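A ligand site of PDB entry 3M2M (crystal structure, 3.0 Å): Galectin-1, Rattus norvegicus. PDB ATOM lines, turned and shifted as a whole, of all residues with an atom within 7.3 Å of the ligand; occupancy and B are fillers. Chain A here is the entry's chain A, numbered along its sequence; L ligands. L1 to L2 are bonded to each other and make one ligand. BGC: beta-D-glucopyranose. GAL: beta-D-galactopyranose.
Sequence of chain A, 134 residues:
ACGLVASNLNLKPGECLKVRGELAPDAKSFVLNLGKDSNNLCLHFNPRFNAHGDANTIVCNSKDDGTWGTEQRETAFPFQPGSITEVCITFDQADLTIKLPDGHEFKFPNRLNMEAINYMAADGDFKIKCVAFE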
ATOM      1  N   SER A  29      12.348  30.576   2.861  1.00  0.00           N
ATOM      2  CA  SER A  29      12.299  29.229   3.432  1.00  0.00           C
ATOM      3  C   SER A  29      12.790  29.258   4.865  1.00  0.00           C
ATOM      4  O   SER A  29      13.559  30.136   5.244  1.00  0.00           O
ATOM      5  CB  SER A  29      13.183  28.265   2.630  1.00  0.00           C
ATOM      6  OG  SER A  29      14.526  28.277   3.099  1.00  0.00           O
ATOM      7  N   VAL A  31      13.748  26.519   8.495  1.00  0.00           N
ATOM      8  CA  VAL A  31      14.073  25.163   8.892  1.00  0.00           C
ATOM      9  C   VAL A  31      13.846  24.840  10.354  1.00  0.00           C
ATOM     10  O   VAL A  31      13.878  25.699  11.224  1.00  0.00           O
ATOM     11  CB  VAL A  31      15.569  24.848   8.563  1.00  0.00           C
ATOM     12  CG1 VAL A  31      15.913  23.402   8.903  1.00  0.00           C
ATOM     13  CG2 VAL A  31      15.825  25.101   7.098  1.00  0.00           C
ATOM     14  N   ASN A  33      15.163  21.486  12.727  1.00  0.00           N
ATOM     15  CA  ASN A  33      15.897  20.228  12.767  1.00  0.00           C
ATOM     16  C   ASN A  33      15.742  19.540  14.111  1.00  0.00           C
ATOM     17  O   ASN A  33      15.808  20.191  15.159  1.00  0.00           O
ATOM     18  CB  ASN A  33      17.387  20.488  12.474  1.00  0.00           C
ATOM     19  CG  ASN A  33      17.628  20.976  11.049  1.00  0.00           C
ATOM     20  OD1 ASN A  33      17.090  20.422  10.103  1.00  0.00           O
ATOM     21  ND2 ASN A  33      18.439  21.994  10.905  1.00  0.00           N
ATOM     22  N   HIS A  44      14.299  16.779   9.225  1.00  0.00           N
ATOM     23  CA  HIS A  44      14.754  18.054   8.677  1.00  0.00           C
ATOM     24  C   HIS A  44      13.513  18.614   8.000  1.00  0.00           C
ATOM     25  O   HIS A  44      13.171  18.232   6.892  1.00  0.00           O
ATOM     26  CB  HIS A  44      15.861  17.838   7.640  1.00  0.00           C
ATOM     27  CG  HIS A  44      16.252  19.089   6.909  1.00  0.00           C
ATOM     28  ND1 HIS A  44      16.883  20.153   7.522  1.00  0.00           N
ATOM     29  CD2 HIS A  44      16.070  19.456   5.615  1.00  0.00           C
ATOM     30  CE1 HIS A  44      17.074  21.116   6.636  1.00  0.00           C
ATOM     31  NE2 HIS A  44      16.582  20.715   5.472  1.00  0.00           N
ATOM     32  N   PHE A  45      12.830  19.520   8.699  1.00  0.00           N
ATOM     33  CA  PHE A  45      11.596  20.131   8.193  1.00  0.00           C
ATOM     34  C   PHE A  45      11.913  21.436   7.467  1.00  0.00           C
ATOM     35  O   PHE A  45      12.058  22.495   8.084  1.00  0.00           O
ATOM     36  CB  PHE A  45      10.657  20.400   9.380  1.00  0.00           C
ATOM     37  CG  PHE A  45       9.309  20.869   8.976  1.00  0.00           C
ATOM     38  CD1 PHE A  45       8.384  19.992   8.444  1.00  0.00           C
ATOM     39  CD2 PHE A  45       8.950  22.213   9.133  1.00  0.00           C
ATOM     40  CE1 PHE A  45       7.118  20.423   8.075  1.00  0.00           C
ATOM     41  CE2 PHE A  45       7.678  22.650   8.763  1.00  0.00           C
ATOM     42  CZ  PHE A  45       6.764  21.743   8.236  1.00  0.00           C
ATOM     43  N   ASN A  46      12.016  21.370   6.146  1.00  0.00           N
ATOM     44  CA  ASN A  46      12.355  22.541   5.342  1.00  0.00           C
ATOM     45  C   ASN A  46      11.289  23.009   4.360  1.00  0.00           C
ATOM     46  O   ASN A  46      11.357  22.687   3.174  1.00  0.00           O
ATOM     47  CB  ASN A  46      13.652  22.277   4.573  1.00  0.00           C
ATOM     48  CG  ASN A  46      14.099  23.468   3.759  1.00  0.00           C
ATOM     49  OD1 ASN A  46      14.855  23.326   2.801  1.00  0.00           O
ATOM     50  ND2 ASN A  46      13.641  24.664   4.140  1.00  0.00           N
ATOM     51  N   ARG A  48       9.783  25.296   1.751  1.00  0.00           N
ATOM     52  CA  ARG A  48      10.371  26.302   0.861  1.00  0.00           C
ATOM     53  C   ARG A  48       9.347  27.127   0.108  1.00  0.00           C
ATOM     54  O   ARG A  48       8.679  26.621  -0.797  1.00  0.00           O
ATOM     55  CB  ARG A  48      11.275  25.609  -0.156  1.00  0.00           C
ATOM     56  CG  ARG A  48      12.393  24.801   0.473  1.00  0.00           C
ATOM     57  CD  ARG A  48      13.074  23.935  -0.568  1.00  0.00           C
ATOM     58  NE  ARG A  48      14.168  23.165   0.012  1.00  0.00           N
ATOM     59  CZ  ARG A  48      14.904  22.291  -0.648  1.00  0.00           C
ATOM     60  NH1 ARG A  48      14.678  22.067  -1.939  1.00  0.00           N
ATOM     61  NH2 ARG A  48      15.872  21.645  -0.025  1.00  0.00           N
ATOM     62  N   ALA A  51      12.888  28.470  -3.016  1.00  0.00           N
ATOM     63  CA  ALA A  51      14.317  28.254  -2.874  1.00  0.00           C
ATOM     64  C   ALA A  51      14.746  26.896  -3.444  1.00  0.00           C
ATOM     65  O   ALA A  51      13.995  25.926  -3.378  1.00  0.00           O
ATOM     66  CB  ALA A  51      14.709  28.346  -1.410  1.00  0.00           C
ATOM     67  N   HIS A  52      15.961  26.861  -3.986  1.00  0.00           N
ATOM     68  CA  HIS A  52      16.537  25.637  -4.561  1.00  0.00           C
ATOM     69  C   HIS A  52      15.737  25.119  -5.752  1.00  0.00           C
ATOM     70  O   HIS A  52      15.894  23.961  -6.142  1.00  0.00           O
ATOM     71  CB  HIS A  52      16.632  24.523  -3.497  1.00  0.00           C
ATOM     72  CG  HIS A  52      17.612  24.806  -2.395  1.00  0.00           C
ATOM     73  ND1 HIS A  52      18.964  24.995  -2.621  1.00  0.00           N
ATOM     74  CD2 HIS A  52      17.432  24.912  -1.053  1.00  0.00           C
ATOM     75  CE1 HIS A  52      19.576  25.213  -1.469  1.00  0.00           C
ATOM     76  NE2 HIS A  52      18.676  25.167  -0.503  1.00  0.00           N
ATOM     77  N   ASP A  54      12.386  25.172  -5.821  1.00  0.00           N
ATOM     78  CA  ASP A  54      11.081  24.705  -5.327  1.00  0.00           C
ATOM     79  C   ASP A  54      10.242  25.857  -4.778  1.00  0.00           C
ATOM     80  O   ASP A  54      10.761  26.724  -4.076  1.00  0.00           O
ATOM     81  CB  ASP A  54      11.292  23.672  -4.225  1.00  0.00           C
ATOM     82  CG  ASP A  54      12.108  22.497  -4.684  1.00  0.00           C
ATOM     83  OD1 ASP A  54      11.666  21.798  -5.628  1.00  0.00           O
ATOM     84  OD2 ASP A  54      13.204  22.287  -4.124  1.00  0.00           O
ATOM     85  N   VAL A  59       9.917  20.257   2.096  1.00  0.00           N
ATOM     86  CA  VAL A  59      10.898  19.201   1.854  1.00  0.00           C
ATOM     87  C   VAL A  59      11.365  18.611   3.173  1.00  0.00           C
ATOM     88  O   VAL A  59      11.847  19.338   4.040  1.00  0.00           O
ATOM     89  CB  VAL A  59      12.104  19.736   1.083  1.00  0.00           C
ATOM     90  CG1 VAL A  59      13.129  18.632   0.886  1.00  0.00           C
ATOM     91  CG2 VAL A  59      11.645  20.274  -0.256  1.00  0.00           C
ATOM     92  N   CYS A  60      11.196  17.301   3.335  1.00  0.00           N
ATOM     93  CA  CYS A  60      11.619  16.619   4.554  1.00  0.00           C
ATOM     94  C   CYS A  60      12.803  15.704   4.256  1.00  0.00           C
ATOM     95  O   CYS A  60      13.004  15.295   3.114  1.00  0.00           O
ATOM     96  CB  CYS A  60      10.478  15.787   5.131  1.00  0.00           C
ATOM     97  SG  CYS A  60       9.165  16.781   5.809  1.00  0.00           S
ATOM     98  N   ASN A  61      13.574  15.389   5.289  1.00  0.00           N
ATOM     99  CA  ASN A  61      14.736  14.514   5.113  1.00  0.00           C
ATOM    100  C   ASN A  61      15.337  14.168   6.472  1.00  0.00           C
ATOM    101  O   ASN A  61      14.925  14.702   7.499  1.00  0.00           O
ATOM    102  CB  ASN A  61      15.791  15.197   4.252  1.00  0.00           C
ATOM    103  CG  ASN A  61      16.662  14.213   3.497  1.00  0.00           C
ATOM    104  OD1 ASN A  61      16.771  13.054   3.888  1.00  0.00           O
ATOM    105  ND2 ASN A  61      17.283  14.675   2.424  1.00  0.00           N
ATOM    106  N   SER A  62      16.312  13.274   6.448  1.00  0.00           N
ATOM    107  CA  SER A  62      17.038  12.870   7.653  1.00  0.00           C
ATOM    108  C   SER A  62      18.532  12.971   7.335  1.00  0.00           C
ATOM    109  O   SER A  62      18.945  12.933   6.178  1.00  0.00           O
ATOM    110  CB  SER A  62      16.678  11.434   8.042  1.00  0.00           C
ATOM    111  OG  SER A  62      17.006  10.512   7.014  1.00  0.00           O
ATOM    112  N   LYS A  63      19.342  13.113   8.373  1.00  0.00           N
ATOM    113  CA  LYS A  63      20.790  13.191   8.195  1.00  0.00           C
ATOM    114  C   LYS A  63      21.483  12.201   9.115  1.00  0.00           C
ATOM    115  O   LYS A  63      21.213  12.133  10.313  1.00  0.00           O
ATOM    116  CB  LYS A  63      21.271  14.609   8.483  1.00  0.00           C
ATOM    117  CG  LYS A  63      22.768  14.735   8.541  1.00  0.00           C
ATOM    118  CD  LYS A  63      23.230  16.183   8.703  1.00  0.00           C
ATOM    119  CE  LYS A  63      23.054  16.991   7.423  1.00  0.00           C
ATOM    120  NZ  LYS A  63      23.783  18.308   7.501  1.00  0.00           N
ATOM    121  N   TRP A  68      23.035  13.509   4.029  1.00  0.00           N
ATOM    122  CA  TRP A  68      21.589  13.514   3.850  1.00  0.00           C
ATOM    123  C   TRP A  68      20.995  12.189   3.352  1.00  0.00           C
ATOM    124  O   TRP A  68      21.679  11.384   2.730  1.00  0.00           O
ATOM    125  CB  TRP A  68      21.177  14.604   2.852  1.00  0.00           C
ATOM    126  CG  TRP A  68      21.502  15.988   3.280  1.00  0.00           C
ATOM    127  CD1 TRP A  68      22.468  16.780   2.752  1.00  0.00           C
ATOM    128  CD2 TRP A  68      20.855  16.755   4.295  1.00  0.00           C
ATOM    129  NE1 TRP A  68      22.467  18.007   3.368  1.00  0.00           N
ATOM    130  CE2 TRP A  68      21.482  18.016   4.318  1.00  0.00           C
ATOM    131  CE3 TRP A  68      19.796  16.506   5.186  1.00  0.00           C
ATOM    132  CZ2 TRP A  68      21.093  19.038   5.200  1.00  0.00           C
ATOM    133  CZ3 TRP A  68      19.405  17.511   6.072  1.00  0.00           C
ATOM    134  CH2 TRP A  68      20.055  18.763   6.067  1.00  0.00           C
ATOM    135  N   GLY A  69      19.707  12.005   3.635  1.00  0.00           N
ATOM    136  CA  GLY A  69      19.023  10.798   3.188  1.00  0.00           C
ATOM    137  C   GLY A  69      18.179  11.107   1.962  1.00  0.00           C
ATOM    138  O   GLY A  69      18.436  12.081   1.253  1.00  0.00           O
ATOM    139  N   THR A  70      17.166  10.291   1.713  1.00  0.00           N
ATOM    140  CA  THR A  70      16.289  10.493   0.569  1.00  0.00           C
ATOM    141  C   THR A  70      15.239  11.549   0.881  1.00  0.00           C
ATOM    142  O   THR A  70      14.615  11.513   1.941  1.00  0.00           O
ATOM    143  CB  THR A  70      15.555   9.206   0.192  1.00  0.00           C
ATOM    144  OG1 THR A  70      16.528   8.218  -0.190  1.00  0.00           O
ATOM    145  CG2 THR A  70      14.575   9.461  -0.955  1.00  0.00           C
ATOM    146  N   GLU A  71      15.028  12.467  -0.045  1.00  0.00           N
ATOM    147  CA  GLU A  71      14.052  13.520   0.146  1.00  0.00           C
ATOM    148  C   GLU A  71      12.607  13.071  -0.088  1.00  0.00           C
ATOM    149  O   GLU A  71      12.320  12.328  -1.029  1.00  0.00           O
ATOM    150  CB  GLU A  71      14.342  14.690  -0.780  1.00  0.00           C
ATOM    151  CG  GLU A  71      15.328  15.688  -0.239  1.00  0.00           C
ATOM    152  CD  GLU A  71      15.538  16.843  -1.200  1.00  0.00           C
ATOM    153  OE1 GLU A  71      14.520  17.383  -1.727  1.00  0.00           O
ATOM    154  OE2 GLU A  71      16.705  17.219  -1.415  1.00  0.00           O
ATOM    155  N   GLN A  72      11.715  13.548   0.779  1.00  0.00           N
ATOM    156  CA  GLN A  72      10.282  13.252   0.692  1.00  0.00           C
ATOM    157  C   GLN A  72       9.616  14.623   0.649  1.00  0.00           C
ATOM    158  O   GLN A  72       9.780  15.436   1.556  1.00  0.00           O
ATOM    159  CB  GLN A  72       9.816  12.457   1.921  1.00  0.00           C
ATOM    160  CG  GLN A  72       8.333  12.153   1.914  1.00  0.00           C
ATOM    161  CD  GLN A  72       7.889  11.397   3.151  1.00  0.00           C
ATOM    162  OE1 GLN A  72       8.458  10.351   3.485  1.00  0.00           O
ATOM    163  NE2 GLN A  72       6.862  11.919   3.823  1.00  0.00           N
ATOM    164  N   ARG A  73       8.860  14.879  -0.403  1.00  0.00           N
ATOM    165  CA  ARG A  73       8.201  16.167  -0.548  1.00  0.00           C
ATOM    166  C   ARG A  73       6.703  16.143  -0.336  1.00  0.00           C
ATOM    167  O   ARG A  73       6.026  15.234  -0.774  1.00  0.00           O
ATOM    168  CB  ARG A  73       8.506  16.729  -1.920  1.00  0.00           C
ATOM    169  CG  ARG A  73       9.958  16.598  -2.250  1.00  0.00           C
ATOM    170  CD  ARG A  73      10.394  17.746  -3.093  1.00  0.00           C
ATOM    171  NE  ARG A  73      11.832  17.746  -3.252  1.00  0.00           N
ATOM    172  CZ  ARG A  73      12.496  18.722  -3.849  1.00  0.00           C
ATOM    173  NH1 ARG A  73      11.828  19.755  -4.332  1.00  0.00           N
ATOM    174  NH2 ARG A  73      13.823  18.661  -3.956  1.00  0.00           N
ATOM    175  N   ASP A 123      16.114  27.496  11.761  1.00  0.00           N
ATOM    176  CA  ASP A 123      16.963  28.212  10.821  1.00  0.00           C
ATOM    177  C   ASP A 123      16.074  28.831   9.744  1.00  0.00           C
ATOM    178  O   ASP A 123      14.880  28.508   9.671  1.00  0.00           O
ATOM    179  CB  ASP A 123      17.953  27.230  10.195  1.00  0.00           C
ATOM    180  CG  ASP A 123      19.142  27.910   9.536  1.00  0.00           C
ATOM    181  OD1 ASP A 123      20.026  27.182   9.019  1.00  0.00           O
ATOM    182  OD2 ASP A 123      19.183  29.160   9.533  1.00  0.00           O
HETATM  183  C2  BGC L   1      18.698  18.708  -3.889  1.00  0.00           C
HETATM  184  C3  BGC L   1      18.488  19.797  -2.844  1.00  0.00           C
HETATM  185  C4  BGC L   1      19.450  19.583  -1.675  1.00  0.00           C
HETATM  186  C5  BGC L   1      20.919  19.471  -2.166  1.00  0.00           C
HETATM  187  C6  BGC L   1      21.892  19.086  -1.063  1.00  0.00           C
HETATM  188  C1  BGC L   1      20.173  18.739  -4.332  1.00  0.00           C
HETATM  189  O1  BGC L   1      20.411  17.766  -5.289  1.00  0.00           O
HETATM  190  O2  BGC L   1      17.843  18.954  -4.998  1.00  0.00           O
HETATM  191  O3  BGC L   1      17.145  19.787  -2.382  1.00  0.00           O
HETATM  192  O4  BGC L   1      19.336  20.713  -0.793  1.00  0.00           O
HETATM  193  O5  BGC L   1      21.031  18.471  -3.206  1.00  0.00           O
HETATM  194  O6  BGC L   1      22.950  20.029  -0.927  1.00  0.00           O
HETATM  195  C1  GAL L   2      19.479  20.505   0.568  1.00  0.00           C
HETATM  196  C2  GAL L   2      19.164  21.830   1.273  1.00  0.00           C
HETATM  197  C3  GAL L   2      19.052  21.662   2.796  1.00  0.00           C
HETATM  198  C4  GAL L   2      18.125  20.488   3.137  1.00  0.00           C
HETATM  199  C5  GAL L   2      18.569  19.228   2.380  1.00  0.00           C
HETATM  200  C6  GAL L   2      17.670  18.015   2.656  1.00  0.00           C
HETATM  201  O2  GAL L   2      20.185  22.772   0.956  1.00  0.00           O
HETATM  202  O3  GAL L   2      18.526  22.863   3.355  1.00  0.00           O
HETATM  203  O4  GAL L   2      16.781  20.831   2.804  1.00  0.00           O
HETATM  204  O5  GAL L   2      18.550  19.481   0.955  1.00  0.00           O
HETATM  205  O6  GAL L   2      17.543  17.169   1.510  1.00  0.00           O
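The side-chain carboxylate of Glu 71 sits at hydrogen-bond distance from an oxygen (O3) of BGC L1, 2.8 Å away. ND2 of Asn 61 is in hydrogen-bond range of O6 of GAL L2 (2.7 Å). A ring nitrogen (NE2) of His 52 sits at hydrogen-bond distance from an oxygen (O2) of GAL L2 (3.2 Å). OD1 of Asn 46 is in hydrogen-bond range of O4 of GAL L2, at 3.2 Å. O4 of GAL L2 is in hydrogen-bond range of NE2 of His 44 (2.7 Å). O4 of GAL L2 sits at hydrogen-bond distance from NH2 of Arg 48, at 3.1 Å.
ND1 of His 44 is in hydrogen-bond range of OD1 of Asn 33. The guanidinium group (NH1) of Arg 73 is in salt-bridge range of the side-chain carboxylate (OD1) of Asp 54, 2.4 Å away. O of Gly 69 sits at hydrogen-bond distance from ND2 of Asn 61. NE of Arg 48 sits at hydrogen-bond distance from OD1 of Asn 46, 2.9 Å away. The backbone carbonyl oxygen of Asn 61 lies within hydrogen-bond range of the backbone NH of His 44 (2.8 Å). The side-chain amide oxygen (OD1) of Asn 61 lies close to the backbone carbonyl oxygen (O) of Thr 70 (3.3 Å). OE1 of Glu 71 lies within salt-bridge range of NH2 of Arg 73, 2.7 Å away. The side-chain carboxylate of Asp 54 lies within salt-bridge range of the guanidinium group of Arg 48 (2.6 Å).
Residues that only touch the ligand: Trp 68 and Arg 73. Hydrophobic or aromatic side chains that line the ligand: His 44, His 52 and Trp 68. The nearest printed residue that does not touch the ligand is Val 59 (4.7 Å).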
